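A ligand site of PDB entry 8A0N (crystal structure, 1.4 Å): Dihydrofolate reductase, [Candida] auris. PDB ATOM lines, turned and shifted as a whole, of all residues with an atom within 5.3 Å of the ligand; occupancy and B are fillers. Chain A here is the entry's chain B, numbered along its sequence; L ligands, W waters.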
ATOM      1  N   ILE A  19     -30.201 -29.622   9.037  1.00  0.00           N
ATOM      2  CA  ILE A  19     -31.200 -29.633  10.110  1.00  0.00           C
ATOM      3  C   ILE A  19     -31.670 -28.199  10.344  1.00  0.00           C
ATOM      4  O   ILE A  19     -30.856 -27.298  10.567  1.00  0.00           O
ATOM      5  CB  ILE A  19     -30.698 -30.334  11.390  1.00  0.00           C
ATOM      6  CG1 ILE A  19     -31.796 -30.351  12.453  1.00  0.00           C
ATOM      7  CG2 ILE A  19     -29.391 -29.699  11.928  1.00  0.00           C
ATOM      8  CD1 ILE A  19     -31.546 -31.349  13.578  1.00  0.00           C
ATOM      9  N   VAL A  20     -32.988 -27.989  10.259  1.00  0.00           N
ATOM     10  CA  VAL A  20     -33.544 -26.643  10.186  1.00  0.00           C
ATOM     11  C   VAL A  20     -34.997 -26.683  10.626  1.00  0.00           C
ATOM     12  O   VAL A  20     -35.675 -27.715  10.488  1.00  0.00           O
ATOM     13  CB  VAL A  20     -33.399 -26.092   8.741  1.00  0.00           C
ATOM     14  CG1 VAL A  20     -34.232 -26.910   7.759  1.00  0.00           C
ATOM     15  CG2 VAL A  20     -33.762 -24.600   8.662  1.00  0.00           C
ATOM     16  N   ALA A  21     -35.484 -25.551  11.138  1.00  0.00           N
ATOM     17  CA  ALA A  21     -36.914 -25.356  11.400  1.00  0.00           C
ATOM     18  C   ALA A  21     -37.444 -24.315  10.420  1.00  0.00           C
ATOM     19  O   ALA A  21     -36.843 -23.264  10.252  1.00  0.00           O
ATOM     20  CB  ALA A  21     -37.134 -24.880  12.843  1.00  0.00           C
ATOM     21  N   ALA A  22     -38.561 -24.634   9.749  1.00  0.00           N
ATOM     22  CA  ALA A  22     -39.140 -23.771   8.722  1.00  0.00           C
ATOM     23  C   ALA A  22     -40.617 -23.531   8.964  1.00  0.00           C
ATOM     24  O   ALA A  22     -41.369 -24.486   9.192  1.00  0.00           O
ATOM     25  CB  ALA A  22     -38.919 -24.352   7.320  1.00  0.00           C
ATOM     26  N   GLY A  28     -40.308 -19.951   5.866  1.00  0.00           N
ATOM     27  CA  GLY A  28     -39.554 -18.895   6.541  1.00  0.00           C
ATOM     28  C   GLY A  28     -38.592 -19.487   7.569  1.00  0.00           C
ATOM     29  O   GLY A  28     -38.971 -20.331   8.392  1.00  0.00           O
ATOM     30  N   ILE A  29     -37.347 -19.021   7.544  1.00  0.00           N
ATOM     31  CA  ILE A  29     -36.303 -19.507   8.446  1.00  0.00           C
ATOM     32  C   ILE A  29     -35.645 -18.411   9.272  1.00  0.00           C
ATOM     33  O   ILE A  29     -34.815 -18.735  10.133  1.00  0.00           O
ATOM     34  CB  ILE A  29     -35.231 -20.341   7.695  1.00  0.00           C
ATOM     35  CG1 ILE A  29     -34.619 -19.521   6.557  1.00  0.00           C
ATOM     36  CG2 ILE A  29     -35.848 -21.666   7.201  1.00  0.00           C
ATOM     37  CD1 ILE A  29     -33.390 -20.151   5.879  1.00  0.00           C
ATOM     38  N   GLY A  30     -35.962 -17.143   9.039  1.00  0.00           N
ATOM     39  CA  GLY A  30     -35.427 -16.091   9.872  1.00  0.00           C
ATOM     40  C   GLY A  30     -36.273 -14.837   9.767  1.00  0.00           C
ATOM     41  O   GLY A  30     -36.989 -14.635   8.778  1.00  0.00           O
ATOM     42  N   ALA A  31     -36.176 -14.005  10.799  1.00  0.00           N
ATOM     43  CA  ALA A  31     -36.832 -12.709  10.777  1.00  0.00           C
ATOM     44  C   ALA A  31     -35.975 -11.754  11.600  1.00  0.00           C
ATOM     45  O   ALA A  31     -35.701 -12.022  12.774  1.00  0.00           O
ATOM     46  CB  ALA A  31     -38.252 -12.786  11.358  1.00  0.00           C
ATOM     47  N   GLY A  33     -32.879 -11.070  11.704  1.00  0.00           N
ATOM     48  CA  GLY A  33     -31.639 -11.622  12.227  1.00  0.00           C
ATOM     49  C   GLY A  33     -31.806 -12.610  13.357  1.00  0.00           C
ATOM     50  O   GLY A  33     -30.807 -13.056  13.931  1.00  0.00           O
ATOM     51  N   SER A  34     -33.036 -13.003  13.675  1.00  0.00           N
ATOM     52  CA  SER A  34     -33.299 -13.920  14.778  1.00  0.00           C
ATOM     53  C   SER A  34     -34.410 -14.858  14.330  1.00  0.00           C
ATOM     54  O   SER A  34     -34.692 -14.986  13.129  1.00  0.00           O
ATOM     55  CB  SER A  34     -33.625 -13.158  16.064  1.00  0.00           C
ATOM     56  OG  SER A  34     -33.532 -14.032  17.164  1.00  0.00           O
ATOM     57  N   LEU A  35     -35.069 -15.496  15.292  1.00  0.00           N
ATOM     58  CA  LEU A  35     -36.130 -16.382  14.919  1.00  0.00           C
ATOM     59  C   LEU A  35     -37.281 -16.075  15.882  1.00  0.00           C
ATOM     60  O   LEU A  35     -37.044 -15.837  17.075  1.00  0.00           O
ATOM     61  CB  LEU A  35     -35.587 -17.799  15.107  1.00  0.00           C
ATOM     62  CG  LEU A  35     -36.333 -19.040  14.701  1.00  0.00           C
ATOM     63  CD1 LEU A  35     -36.458 -18.883  13.188  1.00  0.00           C
ATOM     64  CD2 LEU A  35     -35.483 -20.249  15.005  1.00  0.00           C
ATOM     65  N   TRP A  37     -39.857 -17.804  17.045  1.00  0.00           N
ATOM     66  CA  TRP A  37     -40.297 -18.843  17.953  1.00  0.00           C
ATOM     67  C   TRP A  37     -39.122 -19.330  18.791  1.00  0.00           C
ATOM     68  O   TRP A  37     -37.972 -19.315  18.337  1.00  0.00           O
ATOM     69  CB  TRP A  37     -40.951 -20.020  17.194  1.00  0.00           C
ATOM     70  CG  TRP A  37     -40.084 -20.692  16.161  1.00  0.00           C
ATOM     71  CD1 TRP A  37     -39.178 -21.702  16.368  1.00  0.00           C
ATOM     72  CD2 TRP A  37     -40.079 -20.434  14.750  1.00  0.00           C
ATOM     73  NE1 TRP A  37     -38.598 -22.063  15.172  1.00  0.00           N
ATOM     74  CE2 TRP A  37     -39.128 -21.298  14.162  1.00  0.00           C
ATOM     75  CE3 TRP A  37     -40.775 -19.537  13.935  1.00  0.00           C
ATOM     76  CZ2 TRP A  37     -38.864 -21.298  12.795  1.00  0.00           C
ATOM     77  CZ3 TRP A  37     -40.494 -19.533  12.578  1.00  0.00           C
ATOM     78  CH2 TRP A  37     -39.566 -20.418  12.017  1.00  0.00           C
ATOM     79  N   MET A  63     -21.468 -24.681  10.673  1.00  0.00           N
ATOM     80  CA  MET A  63     -22.247 -23.460  10.836  1.00  0.00           C
ATOM     81  C   MET A  63     -21.514 -22.254  10.272  1.00  0.00           C
ATOM     82  O   MET A  63     -20.283 -22.228  10.205  1.00  0.00           O
ATOM     83  CB  MET A  63     -22.560 -23.281  12.318  1.00  0.00           C
ATOM     84  CG  MET A  63     -21.377 -22.708  13.097  1.00  0.00           C
ATOM     85  SD  MET A  63     -21.666 -22.796  14.871  1.00  0.00           S
ATOM     86  CE  MET A  63     -21.072 -24.444  15.186  1.00  0.00           C
ATOM     87  N   GLY A  64     -22.289 -21.272   9.826  1.00  0.00           N
ATOM     88  CA  GLY A  64     -21.720 -19.995   9.438  1.00  0.00           C
ATOM     89  C   GLY A  64     -21.190 -19.194  10.608  1.00  0.00           C
ATOM     90  O   GLY A  64     -21.550 -19.407  11.778  1.00  0.00           O
ATOM     91  N   ARG A  65     -20.304 -18.259  10.280  1.00  0.00           N
ATOM     92  CA  ARG A  65     -19.673 -17.415  11.298  1.00  0.00           C
ATOM     93  C   ARG A  65     -20.705 -16.701  12.171  1.00  0.00           C
ATOM     94  O   ARG A  65     -20.544 -16.625  13.401  1.00  0.00           O
ATOM     95  CB  ARG A  65     -18.756 -16.409  10.619  1.00  0.00           C
ATOM     96  CG  ARG A  65     -18.029 -15.487  11.599  1.00  0.00           C
ATOM     97  CD  ARG A  65     -17.209 -14.402  10.872  1.00  0.00           C
ATOM     98  NE  ARG A  65     -17.953 -13.765   9.794  1.00  0.00           N
ATOM     99  CZ  ARG A  65     -18.867 -12.819   9.977  1.00  0.00           C
ATOM    100  NH1 ARG A  65     -19.150 -12.384  11.198  1.00  0.00           N
ATOM    101  NH2 ARG A  65     -19.511 -12.302   8.938  1.00  0.00           N
ATOM    102  N   LYS A  66     -21.758 -16.141  11.564  1.00  0.00           N
ATOM    103  CA  LYS A  66     -22.724 -15.397  12.372  1.00  0.00           C
ATOM    104  C   LYS A  66     -23.468 -16.257  13.368  1.00  0.00           C
ATOM    105  O   LYS A  66     -23.796 -15.786  14.467  1.00  0.00           O
ATOM    106  CB  LYS A  66     -23.691 -14.518  11.564  1.00  0.00           C
ATOM    107  CG  LYS A  66     -23.049 -13.476  10.672  1.00  0.00           C
ATOM    108  CD  LYS A  66     -24.213 -12.705  10.048  1.00  0.00           C
ATOM    109  CE  LYS A  66     -23.864 -11.295   9.661  1.00  0.00           C
ATOM    110  NZ  LYS A  66     -22.998 -11.212   8.483  1.00  0.00           N
ATOM    111  N   THR A  67     -23.707 -17.518  13.028  1.00  0.00           N
ATOM    112  CA  THR A  67     -24.386 -18.408  13.963  1.00  0.00           C
ATOM    113  C   THR A  67     -23.456 -18.803  15.110  1.00  0.00           C
ATOM    114  O   THR A  67     -23.865 -18.825  16.266  1.00  0.00           O
ATOM    115  CB  THR A  67     -24.954 -19.605  13.206  1.00  0.00           C
ATOM    116  OG1 THR A  67     -25.989 -19.129  12.314  1.00  0.00           O
ATOM    117  CG2 THR A  67     -25.540 -20.683  14.139  1.00  0.00           C
ATOM    118  N   LEU A  86     -17.651 -21.670   9.261  1.00  0.00           N
ATOM    119  CA  LEU A  86     -17.355 -21.221   7.900  1.00  0.00           C
ATOM    120  C   LEU A  86     -17.308 -19.702   7.833  1.00  0.00           C
ATOM    121  O   LEU A  86     -18.278 -19.020   8.201  1.00  0.00           O
ATOM    122  CB  LEU A  86     -18.384 -21.775   6.905  1.00  0.00           C
ATOM    123  CG  LEU A  86     -18.482 -23.293   6.876  1.00  0.00           C
ATOM    124  CD1 LEU A  86     -19.505 -23.720   5.819  1.00  0.00           C
ATOM    125  CD2 LEU A  86     -17.104 -23.888   6.541  1.00  0.00           C
ATOM    126  N   SER A  87     -16.180 -19.177   7.372  1.00  0.00           N
ATOM    127  CA  SER A  87     -16.012 -17.773   7.037  1.00  0.00           C
ATOM    128  C   SER A  87     -14.965 -17.696   5.936  1.00  0.00           C
ATOM    129  O   SER A  87     -13.924 -18.366   6.035  1.00  0.00           O
ATOM    130  CB  SER A  87     -15.496 -16.970   8.251  1.00  0.00           C
ATOM    131  OG  SER A  87     -14.921 -15.723   7.825  1.00  0.00           O
ATOM    132  N   ARG A  88     -15.234 -16.903   4.909  1.00  0.00           N
ATOM    133  CA  ARG A  88     -14.285 -16.812   3.809  1.00  0.00           C
ATOM    134  C   ARG A  88     -12.966 -16.185   4.225  1.00  0.00           C
ATOM    135  O   ARG A  88     -11.978 -16.315   3.497  1.00  0.00           O
ATOM    136  CB  ARG A  88     -14.939 -16.061   2.650  1.00  0.00           C
ATOM    137  CG  ARG A  88     -16.074 -16.882   2.073  1.00  0.00           C
ATOM    138  CD  ARG A  88     -17.037 -16.031   1.249  1.00  0.00           C
ATOM    139  NE  ARG A  88     -17.764 -15.128   2.130  1.00  0.00           N
ATOM    140  CZ  ARG A  88     -18.814 -14.422   1.764  1.00  0.00           C
ATOM    141  NH1 ARG A  88     -19.290 -14.498   0.531  1.00  0.00           N
ATOM    142  NH2 ARG A  88     -19.390 -13.614   2.646  1.00  0.00           N
ATOM    143  N   LYS A  89     -12.928 -15.530   5.391  1.00  0.00           N
ATOM    144  CA  LYS A  89     -11.709 -14.945   5.960  1.00  0.00           C
ATOM    145  C   LYS A  89     -10.970 -15.916   6.874  1.00  0.00           C
ATOM    146  O   LYS A  89      -9.908 -15.555   7.397  1.00  0.00           O
ATOM    147  CB  LYS A  89     -12.056 -13.664   6.739  1.00  0.00           C
ATOM    148  CG  LYS A  89     -12.620 -12.538   5.865  1.00  0.00           C
ATOM    149  CD  LYS A  89     -13.084 -11.318   6.670  1.00  0.00           C
ATOM    150  CE  LYS A  89     -13.913 -11.656   7.930  1.00  0.00           C
ATOM    151  NZ  LYS A  89     -15.390 -11.809   7.697  1.00  0.00           N
ATOM    152  N   SER A 103     -12.554 -21.995   5.518  1.00  0.00           N
ATOM    153  CA  SER A 103     -12.993 -20.944   4.621  1.00  0.00           C
ATOM    154  C   SER A 103     -14.142 -21.354   3.714  1.00  0.00           C
ATOM    155  O   SER A 103     -14.771 -20.472   3.117  1.00  0.00           O
ATOM    156  CB  SER A 103     -11.794 -20.441   3.799  1.00  0.00           C
ATOM    157  OG  SER A 103     -11.256 -21.465   2.989  1.00  0.00           O
ATOM    158  N   SER A 104     -14.425 -22.641   3.585  1.00  0.00           N
ATOM    159  CA  SER A 104     -15.537 -23.083   2.751  1.00  0.00           C
ATOM    160  C   SER A 104     -15.895 -24.514   3.121  1.00  0.00           C
ATOM    161  O   SER A 104     -15.088 -25.249   3.719  1.00  0.00           O
ATOM    162  CB  SER A 104     -15.156 -23.002   1.271  1.00  0.00           C
ATOM    163  OG  SER A 104     -14.176 -23.965   0.960  1.00  0.00           O
ATOM    164  N   PHE A 105     -17.123 -24.914   2.761  1.00  0.00           N
ATOM    165  CA  PHE A 105     -17.513 -26.298   2.961  1.00  0.00           C
ATOM    166  C   PHE A 105     -16.628 -27.215   2.118  1.00  0.00           C
ATOM    167  O   PHE A 105     -16.267 -28.320   2.558  1.00  0.00           O
ATOM    168  CB  PHE A 105     -18.994 -26.468   2.580  1.00  0.00           C
ATOM    169  CG  PHE A 105     -19.541 -27.831   2.881  1.00  0.00           C
ATOM    170  CD1 PHE A 105     -20.012 -28.636   1.857  1.00  0.00           C
ATOM    171  CD2 PHE A 105     -19.616 -28.290   4.187  1.00  0.00           C
ATOM    172  CE1 PHE A 105     -20.531 -29.896   2.130  1.00  0.00           C
ATOM    173  CE2 PHE A 105     -20.135 -29.549   4.459  1.00  0.00           C
ATOM    174  CZ  PHE A 105     -20.595 -30.354   3.416  1.00  0.00           C
ATOM    175  N   ILE A 130     -26.018 -26.738  10.304  1.00  0.00           N
ATOM    176  CA  ILE A 130     -26.875 -26.209  11.360  1.00  0.00           C
ATOM    177  C   ILE A 130     -27.241 -24.736  11.171  1.00  0.00           C
ATOM    178  O   ILE A 130     -27.842 -24.144  12.081  1.00  0.00           O
ATOM    179  CB  ILE A 130     -26.325 -26.520  12.767  1.00  0.00           C
ATOM    180  CG1 ILE A 130     -25.078 -25.670  13.116  1.00  0.00           C
ATOM    181  CG2 ILE A 130     -26.023 -28.004  12.909  1.00  0.00           C
ATOM    182  CD1 ILE A 130     -24.873 -25.497  14.639  1.00  0.00           C
ATOM    183  N   GLY A 131     -26.913 -24.138  10.042  1.00  0.00           N
ATOM    184  CA  GLY A 131     -27.298 -22.768   9.763  1.00  0.00           C
ATOM    185  C   GLY A 131     -26.098 -21.830   9.747  1.00  0.00           C
ATOM    186  O   GLY A 131     -24.943 -22.267   9.818  1.00  0.00           O
ATOM    187  N   GLY A 132     -26.360 -20.525   9.670  1.00  0.00           N
ATOM    188  CA  GLY A 132     -27.685 -19.936   9.608  1.00  0.00           C
ATOM    189  C   GLY A 132     -28.189 -19.828   8.183  1.00  0.00           C
ATOM    190  O   GLY A 132     -27.823 -20.627   7.337  1.00  0.00           O
ATOM    191  N   SER A 133     -29.029 -18.815   7.922  1.00  0.00           N
ATOM    192  CA  SER A 133     -29.741 -18.756   6.634  1.00  0.00           C
ATOM    193  C   SER A 133     -28.803 -18.726   5.434  1.00  0.00           C
ATOM    194  O   SER A 133     -29.035 -19.425   4.440  1.00  0.00           O
ATOM    195  CB  SER A 133     -30.713 -17.584   6.599  1.00  0.00           C
ATOM    196  OG  SER A 133     -31.631 -17.652   7.677  1.00  0.00           O
ATOM    197  N   GLN A 134     -27.730 -17.929   5.492  1.00  0.00           N
ATOM    198  CA  GLN A 134     -26.843 -17.878   4.331  1.00  0.00           C
ATOM    199  C   GLN A 134     -26.218 -19.245   4.067  1.00  0.00           C
ATOM    200  O   GLN A 134     -26.148 -19.696   2.916  1.00  0.00           O
ATOM    201  CB  GLN A 134     -25.732 -16.843   4.513  1.00  0.00           C
ATOM    202  CG  GLN A 134     -26.173 -15.395   4.363  1.00  0.00           C
ATOM    203  CD  GLN A 134     -24.983 -14.453   4.321  1.00  0.00           C
ATOM    204  OE1 GLN A 134     -24.836 -13.571   5.182  1.00  0.00           O
ATOM    205  NE2 GLN A 134     -24.122 -14.641   3.345  1.00  0.00           N
ATOM    206  N   ILE A 135     -25.734 -19.919   5.121  1.00  0.00           N
ATOM    207  CA  ILE A 135     -25.109 -21.220   4.931  1.00  0.00           C
ATOM    208  C   ILE A 135     -26.142 -22.266   4.494  1.00  0.00           C
ATOM    209  O   ILE A 135     -25.855 -23.108   3.638  1.00  0.00           O
ATOM    210  CB  ILE A 135     -24.323 -21.628   6.191  1.00  0.00           C
ATOM    211  CG1 ILE A 135     -23.137 -20.687   6.404  1.00  0.00           C
ATOM    212  CG2 ILE A 135     -23.847 -23.071   6.115  1.00  0.00           C
ATOM    213  CD1 ILE A 135     -22.271 -20.519   5.212  1.00  0.00           C
ATOM    214  N   TYR A 136     -27.353 -22.213   5.068  1.00  0.00           N
ATOM    215  CA  TYR A 136     -28.409 -23.122   4.636  1.00  0.00           C
ATOM    216  C   TYR A 136     -28.687 -22.972   3.149  1.00  0.00           C
ATOM    217  O   TYR A 136     -28.793 -23.967   2.427  1.00  0.00           O
ATOM    218  CB  TYR A 136     -29.680 -22.778   5.382  1.00  0.00           C
ATOM    219  CG  TYR A 136     -29.840 -23.321   6.788  1.00  0.00           C
ATOM    220  CD1 TYR A 136     -29.466 -24.619   7.139  1.00  0.00           C
ATOM    221  CD2 TYR A 136     -30.494 -22.549   7.738  1.00  0.00           C
ATOM    222  CE1 TYR A 136     -29.664 -25.096   8.442  1.00  0.00           C
ATOM    223  CE2 TYR A 136     -30.709 -23.003   9.021  1.00  0.00           C
ATOM    224  CZ  TYR A 136     -30.331 -24.277   9.375  1.00  0.00           C
ATOM    225  OH  TYR A 136     -30.592 -24.714  10.648  1.00  0.00           O
ATOM    226  N   LEU A 138     -26.832 -21.744   0.801  1.00  0.00           N
ATOM    227  CA  LEU A 138     -25.740 -22.202  -0.038  1.00  0.00           C
ATOM    228  C   LEU A 138     -25.713 -23.722  -0.099  1.00  0.00           C
ATOM    229  O   LEU A 138     -25.725 -24.324  -1.187  1.00  0.00           O
ATOM    230  CB  LEU A 138     -24.427 -21.648   0.542  1.00  0.00           C
ATOM    231  CG  LEU A 138     -23.127 -22.202  -0.001  1.00  0.00           C
ATOM    232  CD1 LEU A 138     -22.907 -21.679  -1.404  1.00  0.00           C
ATOM    233  CD2 LEU A 138     -22.006 -21.778   0.926  1.00  0.00           C
HETATM  234  P1  LIG L   1     -24.834 -17.492   8.903  1.00  0.00           P
HETATM  235  O1  LIG L   1     -25.426 -18.161   7.705  1.00  0.00           O
HETATM  236  O2  LIG L   1     -24.707 -18.225  10.195  1.00  0.00           O
HETATM  237  O3  LIG L   1     -23.290 -16.974   8.622  1.00  0.00           O
HETATM  238  C1  LIG L   1     -23.256 -16.030   7.579  1.00  0.00           C
HETATM  239  C2  LIG L   1     -21.754 -15.811   7.310  1.00  0.00           C
HETATM  240  O4  LIG L   1     -21.228 -16.971   6.701  1.00  0.00           O
HETATM  241  C3  LIG L   1     -21.489 -14.631   6.341  1.00  0.00           C
HETATM  242  O5  LIG L   1     -21.445 -13.405   7.017  1.00  0.00           O
HETATM  243  C4  LIG L   1     -20.081 -14.980   5.873  1.00  0.00           C
HETATM  244  O6  LIG L   1     -19.125 -14.500   6.698  1.00  0.00           O
HETATM  245  C5  LIG L   1     -20.109 -16.575   5.919  1.00  0.00           C
HETATM  246  N1  LIG L   1     -20.253 -17.115   4.562  1.00  0.00           N
HETATM  247  C6  LIG L   1     -21.197 -16.736   3.571  1.00  0.00           C
HETATM  248  N2  LIG L   1     -21.026 -17.406   2.415  1.00  0.00           N
HETATM  249  C7  LIG L   1     -19.932 -18.242   2.655  1.00  0.00           C
HETATM  250  C8  LIG L   1     -19.275 -19.185   1.831  1.00  0.00           C
HETATM  251  N3  LIG L   1     -19.726 -19.360   0.554  1.00  0.00           N
HETATM  252  N4  LIG L   1     -18.200 -19.924   2.288  1.00  0.00           N
HETATM  253  C9  LIG L   1     -17.857 -19.617   3.579  1.00  0.00           C
HETATM  254  N5  LIG L   1     -18.380 -18.752   4.466  1.00  0.00           N
HETATM  255  C10 LIG L   1     -19.434 -18.072   3.974  1.00  0.00           C
HETATM  256  O7  LIG L   1     -25.583 -16.036   9.247  1.00  0.00           O
HETATM  257  P2  LIG L   1     -26.982 -15.530   8.751  1.00  0.00           P
HETATM  258  O8  LIG L   1     -27.056 -14.150   9.301  1.00  0.00           O
HETATM  259  O9  LIG L   1     -27.305 -15.854   7.311  1.00  0.00           O
HETATM  260  O10 LIG L   1     -28.186 -16.484   9.541  1.00  0.00           O
HETATM  261  C11 LIG L   1     -28.688 -15.858  10.635  1.00  0.00           C
HETATM  262  C12 LIG L   1     -30.123 -16.234  10.627  1.00  0.00           C
HETATM  263  O11 LIG L   1     -30.206 -17.682  10.583  1.00  0.00           O
HETATM  264  C13 LIG L   1     -30.866 -15.752  11.891  1.00  0.00           C
HETATM  265  O12 LIG L   1     -32.085 -15.199  11.452  1.00  0.00           O
HETATM  266  C14 LIG L   1     -31.116 -17.075  12.603  1.00  0.00           C
HETATM  267  O13 LIG L   1     -32.322 -17.068  13.374  1.00  0.00           O
HETATM  268  C15 LIG L   1     -31.319 -18.008  11.369  1.00  0.00           C
HETATM  269  N6  LIG L   1     -31.274 -19.416  11.784  1.00  0.00           N
HETATM  270  C16 LIG L   1     -32.377 -20.205  11.570  1.00  0.00           C
HETATM  271  C17 LIG L   1     -32.426 -21.481  12.016  1.00  0.00           C
HETATM  272  C18 LIG L   1     -33.640 -22.250  11.739  1.00  0.00           C
HETATM  273  O14 LIG L   1     -33.787 -23.408  12.122  1.00  0.00           O
HETATM  274  N7  LIG L   1     -34.650 -21.622  11.029  1.00  0.00           N
HETATM  275  C19 LIG L   1     -31.296 -22.135  12.752  1.00  0.00           C
HETATM  276  C20 LIG L   1     -30.139 -21.205  12.897  1.00  0.00           C
HETATM  277  C21 LIG L   1     -30.159 -19.956  12.442  1.00  0.00           C
HETATM  278  P3  LIG L   1     -17.585 -14.163   5.860  1.00  0.00           P
HETATM  279  O15 LIG L   1     -17.956 -12.890   5.165  1.00  0.00           O
HETATM  280  O16 LIG L   1     -17.315 -15.363   4.956  1.00  0.00           O
HETATM  281  O17 LIG L   1     -16.756 -14.029   7.110  1.00  0.00           O
HETATM  282  O   HOH W   1     -26.716 -15.103  13.312  1.00  0.00           O
HETATM  283  O   HOH W   2     -32.303 -14.746   8.689  1.00  0.00           O
HETATM  284  O   HOH W   3     -27.936 -17.741  13.710  1.00  0.00           O
HETATM  285  O   HOH W   4     -18.806 -22.937   1.891  1.00  0.00           O
HETATM  286  O   HOH W   5     -18.779 -21.403  -1.622  1.00  0.00           O
HETATM  287  O   HOH W   6     -33.972 -23.884  14.902  1.00  0.00           O
HETATM  288  O   HOH W   7     -26.464 -12.468   7.186  1.00  0.00           O
HETATM  289  O   HOH W   8     -28.338 -12.277  10.487  1.00  0.00           O
HETATM  290  O   HOH W   9     -29.249 -14.215   6.359  1.00  0.00           O
HETATM  291  O   HOH W  10     -16.103 -19.823   0.204  1.00  0.00           O
HETATM  292  O   HOH W  11     -32.849 -25.955  13.499  1.00  0.00           O
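CG2 of Val 20 touches O14 of the ligand (3.7 Å).
Gly 30 touches the ligand.
C of Gly 33 touches O12 of the ligand (3.2 Å).
N of Leu 35 touches O13 of the ligand (3.7 Å).
Gly 64 touches the ligand (CA to O3, 3.5 Å).
Leu 86 touches the ligand (C to N5, 3.7 Å).
Ser 103 touches the ligand (O to C9, 3.2 Å).
Ile 130 touches the ligand.
C of Gly 131 touches O2 of the ligand (3.9 Å).
OH of Tyr 136 touches C19 of the ligand, at 3.4 Å.
CD2 of Leu 138 touches N3 of the ligand, 3.3 Å away.
Hydrophobic or aromatic side chains that line the ligand: Val 20, Ala 21, Ile 29, Leu 35, Leu 86, Ile 135, Tyr 136 and Leu 138.
24 residues have an atom within 4 Å of the ligand: Val 20, Ala 21, Ile 29, Gly 30, Gly 33, Ser 34, Leu 35, Gly 64, Arg 65, Lys 66, Thr 67, Leu 86, Ser 87, Arg 88, Lys 89, Ser 103, Ile 130, Gly 131, Gly 132, Ser 133, Gln 134, Ile 135, Tyr 136 and Leu 138.
O2 of the ligand is in hydrogen-bond range of N of Gly 132, 2.9 Å away.
The backbone NH (N) of Ala 21 lies within hydrogen-bond range of an oxygen (O14) of the ligand (2.9 Å).
The backbone carbonyl oxygen (O) of Ser 34 is in hydrogen-bond range of an oxygen (O12) of the ligand (3.1 Å).
An oxygen (O2) of the ligand lies within hydrogen-bond range of the backbone NH of Thr 67 (3.1 Å).
OG of Ser 133 lies within hydrogen-bond range of O11 of the ligand, 3.2 Å away.
An oxygen (O1) of the ligand sits at hydrogen-bond distance from the backbone NH (N) of Ile 135 (3.1 Å).
NE of Arg 88 is in salt-bridge range of O16 of the ligand, 2.9 Å away.
The backbone NH of Arg 88 is in hydrogen-bond range of an oxygen (O16) of the ligand (2.6 Å).
O3 of the ligand is in hydrogen-bond range of N of Lys 66 (3.4 Å).
An oxygen (O12) of the ligand is in hydrogen-bond range of the backbone NH (N) of Ser 34 (3.3 Å).
O2 of the ligand lies within hydrogen-bond range of OG1 of Thr 67 (2.6 Å).
The backbone NH of Gln 134 lies within hydrogen-bond range of an oxygen (O9) of the ligand (2.8 Å).
N of Ser 133 is in hydrogen-bond range of O10 of the ligand (3.0 Å).
The guanidinium group of Arg 65 lies within salt-bridge range of an oxygen (O17) of the ligand (3.0 Å).
An oxygen (O17) of the ligand is in salt-bridge range of the side-chain amino group of Lys 89, 2.7 Å away.
The side-chain hydroxyl (OG) of Ser 87 sits at hydrogen-bond distance from an oxygen (O17) of the ligand (2.6 Å).
NZ of Lys 66 is in hydrogen-bond range of O5 of the ligand (3.1 Å).
N7 of the ligand sits at hydrogen-bond distance from O of Ile 29 (3.0 Å).
O of Ala 21 is in hydrogen-bond range of N7 of the ligand, 2.8 Å away.
Water W7 bridges an oxygen (O8) of the ligand and the side-chain amide oxygen of Gln 134.
Water W2 lies within hydrogen-bond range of an oxygen (O12) of the ligand (2.8 Å) and the side-chain hydroxyl of Ser 133 (3.1 Å).
Water W10 lies within hydrogen-bond range of a nitrogen (N4) of the ligand (3.0 Å) and the backbone carbonyl oxygen (O) of Ser 103 (3.3 Å).
Water W4 lies within hydrogen-bond range of the backbone NH of Phe 105 (2.7 Å) and a nitrogen (N4) of the ligand (3.1 Å).
O of Gly 131 sits at hydrogen-bond distance from N of Gly 64 (2.8 Å).
The backbone carbonyl oxygen of Ile 130 is in hydrogen-bond range of the side-chain hydroxyl of Tyr 136 (3.2 Å).
The backbone carbonyl oxygen (O) of Ile 19 sits at hydrogen-bond distance from the side-chain hydroxyl (OH) of Tyr 136, 2.6 Å away.
N of Arg 65 lies within hydrogen-bond range of O of Leu 86 (3.0 Å).
OG of Ser 87 lies close to N of Lys 89 (3.2 Å).
The backbone NH of Leu 86 sits at hydrogen-bond distance from the backbone carbonyl oxygen of Met 63 (2.9 Å).
The backbone NH (N) of Gly 132 is in hydrogen-bond range of the side-chain hydroxyl (OG1) of Thr 67 (3.0 Å).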
